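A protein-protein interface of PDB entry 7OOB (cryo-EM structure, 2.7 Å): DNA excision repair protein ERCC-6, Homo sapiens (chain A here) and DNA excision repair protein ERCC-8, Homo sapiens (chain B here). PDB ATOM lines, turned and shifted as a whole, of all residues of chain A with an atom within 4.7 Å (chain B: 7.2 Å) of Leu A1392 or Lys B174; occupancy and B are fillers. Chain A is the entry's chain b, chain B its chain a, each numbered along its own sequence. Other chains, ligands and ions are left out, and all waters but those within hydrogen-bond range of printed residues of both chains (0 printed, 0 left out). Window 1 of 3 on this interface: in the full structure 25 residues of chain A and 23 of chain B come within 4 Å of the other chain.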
ATOM      1  N   ASP A 739      14.371   0.367 -25.458  1.00  0.00           N
ATOM      2  CA  ASP A 739      15.150   1.532 -25.053  1.00  0.00           C
ATOM      3  C   ASP A 739      16.079   1.981 -26.167  1.00  0.00           C
ATOM      4  O   ASP A 739      16.183   3.178 -26.457  1.00  0.00           O
ATOM      5  CB  ASP A 739      15.964   1.213 -23.803  1.00  0.00           C
ATOM      6  CG  ASP A 739      15.204   1.482 -22.530  1.00  0.00           C
ATOM      7  OD1 ASP A 739      14.827   2.651 -22.303  1.00  0.00           O
ATOM      8  OD2 ASP A 739      14.993   0.529 -21.752  1.00  0.00           O
ATOM      9  N   LEU A1387      22.809  11.373 -14.258  1.00  0.00           N
ATOM     10  CA  LEU A1387      22.363  10.350 -13.325  1.00  0.00           C
ATOM     11  C   LEU A1387      23.384  10.200 -12.206  1.00  0.00           C
ATOM     12  O   LEU A1387      24.588  10.124 -12.456  1.00  0.00           O
ATOM     13  CB  LEU A1387      22.170   9.022 -14.054  1.00  0.00           C
ATOM     14  CG  LEU A1387      21.176   9.016 -15.217  1.00  0.00           C
ATOM     15  CD1 LEU A1387      21.151   7.642 -15.860  1.00  0.00           C
ATOM     16  CD2 LEU A1387      19.777   9.428 -14.774  1.00  0.00           C
ATOM     17  N   SER A1389      24.553   7.932 -10.256  1.00  0.00           N
ATOM     18  CA  SER A1389      25.181   6.641  -9.985  1.00  0.00           C
ATOM     19  C   SER A1389      24.340   5.710  -9.116  1.00  0.00           C
ATOM     20  O   SER A1389      24.842   4.668  -8.686  1.00  0.00           O
ATOM     21  CB  SER A1389      26.547   6.819  -9.322  1.00  0.00           C
ATOM     22  OG  SER A1389      26.392   7.022  -7.929  1.00  0.00           O
ATOM     23  N   SER A1390      23.089   6.052  -8.834  1.00  0.00           N
ATOM     24  CA  SER A1390      22.223   5.248  -7.981  1.00  0.00           C
ATOM     25  C   SER A1390      20.935   4.861  -8.676  1.00  0.00           C
ATOM     26  O   SER A1390      20.492   3.716  -8.555  1.00  0.00           O
ATOM     27  CB  SER A1390      21.909   6.011  -6.691  1.00  0.00           C
ATOM     28  OG  SER A1390      23.096   6.259  -5.959  1.00  0.00           O
ATOM     29  N   SER A1391      20.325   5.787  -9.413  1.00  0.00           N
ATOM     30  CA  SER A1391      19.363   5.381 -10.427  1.00  0.00           C
ATOM     31  C   SER A1391      20.038   4.489 -11.455  1.00  0.00           C
ATOM     32  O   SER A1391      19.479   3.470 -11.874  1.00  0.00           O
ATOM     33  CB  SER A1391      18.758   6.613 -11.099  1.00  0.00           C
ATOM     34  OG  SER A1391      19.766   7.397 -11.711  1.00  0.00           O
ATOM     35  N   LEU A1392      21.263   4.842 -11.843  1.00  0.00           N
ATOM     36  CA  LEU A1392      22.013   4.034 -12.796  1.00  0.00           C
ATOM     37  C   LEU A1392      22.316   2.656 -12.226  1.00  0.00           C
ATOM     38  O   LEU A1392      22.038   1.628 -12.862  1.00  0.00           O
ATOM     39  CB  LEU A1392      23.306   4.759 -13.163  1.00  0.00           C
ATOM     40  CG  LEU A1392      24.213   4.107 -14.201  1.00  0.00           C
ATOM     41  CD1 LEU A1392      23.509   3.997 -15.536  1.00  0.00           C
ATOM     42  CD2 LEU A1392      25.485   4.919 -14.329  1.00  0.00           C
ATOM     43  N   LEU A1393      22.881   2.611 -11.021  1.00  0.00           N
ATOM     44  CA  LEU A1393      23.189   1.320 -10.431  1.00  0.00           C
ATOM     45  C   LEU A1393      21.920   0.529 -10.162  1.00  0.00           C
ATOM     46  O   LEU A1393      21.878  -0.669 -10.433  1.00  0.00           O
ATOM     47  CB  LEU A1393      24.000   1.496  -9.146  1.00  0.00           C
ATOM     48  CG  LEU A1393      25.497   1.794  -9.287  1.00  0.00           C
ATOM     49  CD1 LEU A1393      26.099   1.993  -7.913  1.00  0.00           C
ATOM     50  CD2 LEU A1393      26.248   0.693 -10.013  1.00  0.00           C
ATOM     51  N   ALA A1394      20.868   1.185  -9.668  1.00  0.00           N
ATOM     52  CA  ALA A1394      19.614   0.478  -9.423  1.00  0.00           C
ATOM     53  C   ALA A1394      19.078  -0.145 -10.704  1.00  0.00           C
ATOM     54  O   ALA A1394      18.603  -1.287 -10.697  1.00  0.00           O
ATOM     55  CB  ALA A1394      18.583   1.429  -8.819  1.00  0.00           C
ATOM     56  N   LYS A1395      19.150   0.590 -11.817  1.00  0.00           N
ATOM     57  CA  LYS A1395      18.742   0.027 -13.099  1.00  0.00           C
ATOM     58  C   LYS A1395      19.608  -1.168 -13.470  1.00  0.00           C
ATOM     59  O   LYS A1395      19.114  -2.152 -14.036  1.00  0.00           O
ATOM     60  CB  LYS A1395      18.813   1.103 -14.182  1.00  0.00           C
ATOM     61  CG  LYS A1395      17.696   2.126 -14.092  1.00  0.00           C
ATOM     62  CD  LYS A1395      17.832   3.215 -15.142  1.00  0.00           C
ATOM     63  CE  LYS A1395      16.695   4.218 -15.027  1.00  0.00           C
ATOM     64  NZ  LYS A1395      16.723   5.243 -16.105  1.00  0.00           N
ATOM     65  N   MET A1396      20.903  -1.104 -13.166  1.00  0.00           N
ATOM     66  CA  MET A1396      21.776  -2.237 -13.465  1.00  0.00           C
ATOM     67  C   MET A1396      21.403  -3.465 -12.640  1.00  0.00           C
ATOM     68  O   MET A1396      21.345  -4.582 -13.167  1.00  0.00           O
ATOM     69  CB  MET A1396      23.230  -1.855 -13.217  1.00  0.00           C
ATOM     70  CG  MET A1396      23.850  -1.100 -14.355  1.00  0.00           C
ATOM     71  SD  MET A1396      25.293  -0.175 -13.834  1.00  0.00           S
ATOM     72  CE  MET A1396      25.586   0.755 -15.320  1.00  0.00           C
ATOM     73  N   TYR B 108      33.369   6.942 -12.672  1.00  0.00           N
ATOM     74  CA  TYR B 108      32.218   7.549 -13.280  1.00  0.00           C
ATOM     75  C   TYR B 108      32.321   9.048 -13.059  1.00  0.00           C
ATOM     76  O   TYR B 108      32.422   9.478 -11.905  1.00  0.00           O
ATOM     77  CB  TYR B 108      30.951   7.017 -12.654  1.00  0.00           C
ATOM     78  CG  TYR B 108      29.706   7.752 -13.082  1.00  0.00           C
ATOM     79  CD1 TYR B 108      29.354   7.833 -14.419  1.00  0.00           C
ATOM     80  CD2 TYR B 108      28.867   8.332 -12.149  1.00  0.00           C
ATOM     81  CE1 TYR B 108      28.215   8.487 -14.817  1.00  0.00           C
ATOM     82  CE2 TYR B 108      27.722   8.990 -12.535  1.00  0.00           C
ATOM     83  CZ  TYR B 108      27.401   9.063 -13.873  1.00  0.00           C
ATOM     84  OH  TYR B 108      26.261   9.716 -14.272  1.00  0.00           O
ATOM     85  N   MET B 114      30.311   4.910  -8.473  1.00  0.00           N
ATOM     86  CA  MET B 114      30.434   3.875  -9.488  1.00  0.00           C
ATOM     87  C   MET B 114      31.706   4.123 -10.283  1.00  0.00           C
ATOM     88  O   MET B 114      32.098   5.273 -10.493  1.00  0.00           O
ATOM     89  CB  MET B 114      29.182   3.860 -10.398  1.00  0.00           C
ATOM     90  CG  MET B 114      29.208   2.868 -11.569  1.00  0.00           C
ATOM     91  SD  MET B 114      30.103   3.394 -13.039  1.00  0.00           S
ATOM     92  CE  MET B 114      28.916   4.547 -13.720  1.00  0.00           C
ATOM     93  N   VAL B 126      31.224  -2.852 -14.765  1.00  0.00           N
ATOM     94  CA  VAL B 126      30.784  -1.688 -14.009  1.00  0.00           C
ATOM     95  C   VAL B 126      30.722  -2.096 -12.547  1.00  0.00           C
ATOM     96  O   VAL B 126      30.115  -3.117 -12.204  1.00  0.00           O
ATOM     97  CB  VAL B 126      29.418  -1.180 -14.505  1.00  0.00           C
ATOM     98  CG1 VAL B 126      28.974   0.026 -13.702  1.00  0.00           C
ATOM     99  CG2 VAL B 126      29.478  -0.831 -15.977  1.00  0.00           C
ATOM    100  N   ALA B 135      27.950  -4.237 -10.947  1.00  0.00           N
ATOM    101  CA  ALA B 135      26.575  -3.954 -11.313  1.00  0.00           C
ATOM    102  C   ALA B 135      26.245  -4.420 -12.718  1.00  0.00           C
ATOM    103  O   ALA B 135      25.075  -4.696 -13.010  1.00  0.00           O
ATOM    104  CB  ALA B 135      26.302  -2.454 -11.203  1.00  0.00           C
ATOM    105  N   ASP B 136      27.246  -4.534 -13.585  1.00  0.00           N
ATOM    106  CA  ASP B 136      27.012  -4.882 -14.974  1.00  0.00           C
ATOM    107  C   ASP B 136      28.306  -5.408 -15.568  1.00  0.00           C
ATOM    108  O   ASP B 136      29.402  -5.079 -15.107  1.00  0.00           O
ATOM    109  CB  ASP B 136      26.509  -3.675 -15.771  1.00  0.00           C
ATOM    110  CG  ASP B 136      25.722  -4.073 -16.999  1.00  0.00           C
ATOM    111  OD1 ASP B 136      25.670  -5.278 -17.315  1.00  0.00           O
ATOM    112  OD2 ASP B 136      25.156  -3.176 -17.655  1.00  0.00           O
ATOM    113  N   PHE B 138      29.803  -6.030 -19.651  1.00  0.00           N
ATOM    114  CA  PHE B 138      29.660  -5.960 -21.098  1.00  0.00           C
ATOM    115  C   PHE B 138      30.732  -6.877 -21.665  1.00  0.00           C
ATOM    116  O   PHE B 138      31.925  -6.558 -21.613  1.00  0.00           O
ATOM    117  CB  PHE B 138      29.802  -4.528 -21.597  1.00  0.00           C
ATOM    118  CG  PHE B 138      28.731  -3.610 -21.093  1.00  0.00           C
ATOM    119  CD1 PHE B 138      28.837  -3.021 -19.849  1.00  0.00           C
ATOM    120  CD2 PHE B 138      27.613  -3.341 -21.861  1.00  0.00           C
ATOM    121  CE1 PHE B 138      27.854  -2.180 -19.381  1.00  0.00           C
ATOM    122  CE2 PHE B 138      26.628  -2.499 -21.398  1.00  0.00           C
ATOM    123  CZ  PHE B 138      26.750  -1.918 -20.156  1.00  0.00           C
ATOM    124  N   MET B 149      34.466   6.939 -20.585  1.00  0.00           N
ATOM    125  CA  MET B 149      33.181   7.583 -20.382  1.00  0.00           C
ATOM    126  C   MET B 149      33.354   9.072 -20.608  1.00  0.00           C
ATOM    127  O   MET B 149      34.403   9.641 -20.294  1.00  0.00           O
ATOM    128  CB  MET B 149      32.654   7.330 -18.973  1.00  0.00           C
ATOM    129  CG  MET B 149      32.049   5.967 -18.797  1.00  0.00           C
ATOM    130  SD  MET B 149      31.443   5.650 -17.136  1.00  0.00           S
ATOM    131  CE  MET B 149      32.985   5.582 -16.236  1.00  0.00           C
ATOM    132  N   LYS B 155      23.779  14.080 -20.233  1.00  0.00           N
ATOM    133  CA  LYS B 155      22.640  13.498 -20.936  1.00  0.00           C
ATOM    134  C   LYS B 155      22.799  11.998 -21.166  1.00  0.00           C
ATOM    135  O   LYS B 155      21.966  11.209 -20.711  1.00  0.00           O
ATOM    136  CB  LYS B 155      22.442  14.214 -22.278  1.00  0.00           C
ATOM    137  CG  LYS B 155      22.045  15.674 -22.144  1.00  0.00           C
ATOM    138  CD  LYS B 155      21.900  16.340 -23.502  1.00  0.00           C
ATOM    139  CE  LYS B 155      21.478  17.792 -23.358  1.00  0.00           C
ATOM    140  NZ  LYS B 155      21.343  18.474 -24.675  1.00  0.00           N
ATOM    141  N   HIS B 156      23.866  11.590 -21.849  1.00  0.00           N
ATOM    142  CA  HIS B 156      24.083  10.199 -22.223  1.00  0.00           C
ATOM    143  C   HIS B 156      25.143   9.589 -21.321  1.00  0.00           C
ATOM    144  O   HIS B 156      25.973  10.298 -20.749  1.00  0.00           O
ATOM    145  CB  HIS B 156      24.512  10.076 -23.691  1.00  0.00           C
ATOM    146  CG  HIS B 156      25.934  10.478 -23.954  1.00  0.00           C
ATOM    147  ND1 HIS B 156      27.006   9.657 -23.685  1.00  0.00           N
ATOM    148  CD2 HIS B 156      26.457  11.614 -24.470  1.00  0.00           C
ATOM    149  CE1 HIS B 156      28.126  10.267 -24.020  1.00  0.00           C
ATOM    150  NE2 HIS B 156      27.822  11.458 -24.500  1.00  0.00           N
ATOM    151  N   CYS B 157      25.095   8.267 -21.177  1.00  0.00           N
ATOM    152  CA  CYS B 157      26.067   7.581 -20.339  1.00  0.00           C
ATOM    153  C   CYS B 157      26.704   6.455 -21.148  1.00  0.00           C
ATOM    154  O   CYS B 157      26.739   5.298 -20.720  1.00  0.00           O
ATOM    155  CB  CYS B 157      25.398   7.077 -19.062  1.00  0.00           C
ATOM    156  SG  CYS B 157      26.534   6.301 -17.911  1.00  0.00           S
ATOM    157  N   LEU B 158      27.156   6.792 -22.351  1.00  0.00           N
ATOM    158  CA  LEU B 158      27.839   5.851 -23.223  1.00  0.00           C
ATOM    159  C   LEU B 158      29.288   5.660 -22.798  1.00  0.00           C
ATOM    160  O   LEU B 158      29.959   6.602 -22.370  1.00  0.00           O
ATOM    161  CB  LEU B 158      27.799   6.346 -24.668  1.00  0.00           C
ATOM    162  CG  LEU B 158      26.456   6.310 -25.398  1.00  0.00           C
ATOM    163  CD1 LEU B 158      26.572   7.055 -26.715  1.00  0.00           C
ATOM    164  CD2 LEU B 158      25.997   4.880 -25.636  1.00  0.00           C
ATOM    165  N   CYS B 171      28.690   1.365 -25.440  1.00  0.00           N
ATOM    166  CA  CYS B 171      27.869   0.657 -24.466  1.00  0.00           C
ATOM    167  C   CYS B 171      27.088   1.679 -23.656  1.00  0.00           C
ATOM    168  O   CYS B 171      27.685   2.519 -22.981  1.00  0.00           O
ATOM    169  CB  CYS B 171      28.739  -0.197 -23.544  1.00  0.00           C
ATOM    170  SG  CYS B 171      29.837  -1.335 -24.405  1.00  0.00           S
ATOM    171  N   ASP B 172      25.766   1.587 -23.694  1.00  0.00           N
ATOM    172  CA  ASP B 172      24.912   2.493 -22.934  1.00  0.00           C
ATOM    173  C   ASP B 172      24.693   1.887 -21.555  1.00  0.00           C
ATOM    174  O   ASP B 172      24.107   0.811 -21.431  1.00  0.00           O
ATOM    175  CB  ASP B 172      23.586   2.718 -23.661  1.00  0.00           C
ATOM    176  CG  ASP B 172      22.979   4.084 -23.380  1.00  0.00           C
ATOM    177  OD1 ASP B 172      23.708   5.013 -22.974  1.00  0.00           O
ATOM    178  OD2 ASP B 172      21.756   4.231 -23.576  1.00  0.00           O
ATOM    179  N   LEU B 173      25.186   2.562 -20.518  1.00  0.00           N
ATOM    180  CA  LEU B 173      24.990   2.062 -19.163  1.00  0.00           C
ATOM    181  C   LEU B 173      23.526   2.150 -18.757  1.00  0.00           C
ATOM    182  O   LEU B 173      22.966   1.196 -18.206  1.00  0.00           O
ATOM    183  CB  LEU B 173      25.878   2.835 -18.192  1.00  0.00           C
ATOM    184  CG  LEU B 173      27.398   2.800 -18.390  1.00  0.00           C
ATOM    185  CD1 LEU B 173      28.118   3.205 -17.112  1.00  0.00           C
ATOM    186  CD2 LEU B 173      27.892   1.433 -18.845  1.00  0.00           C
ATOM    187  N   LYS B 174      22.885   3.293 -19.013  1.00  0.00           N
ATOM    188  CA  LYS B 174      21.429   3.333 -19.076  1.00  0.00           C
ATOM    189  C   LYS B 174      21.028   2.305 -20.125  1.00  0.00           C
ATOM    190  O   LYS B 174      21.818   2.059 -21.041  1.00  0.00           O
ATOM    191  CB  LYS B 174      20.931   4.742 -19.413  1.00  0.00           C
ATOM    192  CG  LYS B 174      19.421   4.898 -19.407  1.00  0.00           C
ATOM    193  CD  LYS B 174      19.003   6.331 -19.673  1.00  0.00           C
ATOM    194  CE  LYS B 174      17.486   6.471 -19.679  1.00  0.00           C
ATOM    195  NZ  LYS B 174      16.855   5.716 -20.799  1.00  0.00           N
ATOM    196  N   SER B 175      19.780   1.823 -20.102  1.00  0.00           N
ATOM    197  CA  SER B 175      19.452   0.421 -20.374  1.00  0.00           C
ATOM    198  C   SER B 175      20.438  -0.263 -21.312  1.00  0.00           C
ATOM    199  O   SER B 175      20.670   0.198 -22.434  1.00  0.00           O
ATOM    200  CB  SER B 175      18.048   0.335 -20.974  1.00  0.00           C
ATOM    201  OG  SER B 175      17.513  -0.971 -20.858  1.00  0.00           O
ATOM    202  N   GLY B 176      20.996  -1.383 -20.855  1.00  0.00           N
ATOM    203  CA  GLY B 176      22.262  -1.876 -21.363  1.00  0.00           C
ATOM    204  C   GLY B 176      22.257  -2.201 -22.838  1.00  0.00           C
ATOM    205  O   GLY B 176      21.753  -3.250 -23.242  1.00  0.00           O
ATOM    206  N   SER B 177      22.871  -1.337 -23.643  1.00  0.00           N
ATOM    207  CA  SER B 177      22.830  -1.443 -25.100  1.00  0.00           C
ATOM    208  C   SER B 177      24.263  -1.406 -25.620  1.00  0.00           C
ATOM    209  O   SER B 177      24.846  -0.331 -25.774  1.00  0.00           O
ATOM    210  CB  SER B 177      21.991  -0.321 -25.701  1.00  0.00           C
ATOM    211  OG  SER B 177      20.668  -0.356 -25.200  1.00  0.00           O
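Among the printed residues, pairs that only touch across the chains: Ser A1389 with Tyr B108 (3.96 Å), Leu A1392 with Met B114 (3.5 Å), Leu A1392 with Cys B157 (3.98 Å), Leu A1392 with Leu B173 (3.7 Å), Leu A1392 with Lys B174 (3.6 Å), Leu A1393 with Met B114 (3.99 Å), Leu A1393 with Ala B135 (3.4 Å), Lys A1395 with Lys B174 (3.9 Å), Met A1396 with Val B126 (3.7 Å), Met A1396 with Ala B135 (3.4 Å), Met A1396 with Asp B136 (3.96 Å) and Met A1396 with Leu B173 (3.6 Å).
The backbone NH (N) of Tyr B108 sits close to the backbone carbonyl oxygen (O) of Met B114, 3.0 Å away. N of Ala B135 sits at hydrogen-bond distance from O of Val B126 (2.7 Å). The backbone carbonyl oxygen (O) of Asp B136 lies within hydrogen-bond range of the backbone NH (N) of Val B126 (2.9 Å). The backbone carbonyl oxygen of Cys B157 lies within hydrogen-bond range of the backbone NH of Leu B173 (3.2 Å). The backbone carbonyl oxygen of Ser B175 sits at hydrogen-bond distance from the side-chain hydroxyl of Ser B177, at 2.8 Å.
Of the 18 printed residues of chain B, 9 touch a printed residue of chain A. Of the 10 printed residues of chain A, 7 touch a printed residue of chain B. Printed residues of chain A that touch a printed residue of chain B: Asp A739, Leu A1387, Ser A1389, Leu A1392, Leu A1393, Lys A1395 and Met A1396.
The side-chain amino group (NZ) of Lys B174 lies within salt-bridge range of the side-chain carboxylate (OD1) of Asp A739 (3.97 Å). OD2 of Asp A739 is in hydrogen-bond range of OG of Ser B175 (3.1 Å). The backbone carbonyl oxygen of Leu A1387 is in hydrogen-bond range of the side-chain hydroxyl of Tyr B108 (2.5 Å).
Lys B174 touches just these residues of chain A: Asp A739 (3.97 Å), Leu A1392 (3.6 Å) and Lys A1395 (3.9 Å). Printed residues of chain A within 4 Å of Val B126: Met A1396 (3.7 Å). Printed residues of chain A within 4 Å of Ala B135: Leu A1393 and Met A1396. Of the printed residues of chain A, Tyr B108 touches Leu A1387 (2.5 Å) and Ser A1389 (3.96 Å). Of the printed residues of chain A, Ser B175 touches Asp A739 (3.1 Å). Of the printed residues of chain B, Leu A1387 touches Tyr B108. Phe B138 touches none of the printed residues of chain A. Ser B177 touches none of the printed residues of chain A.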
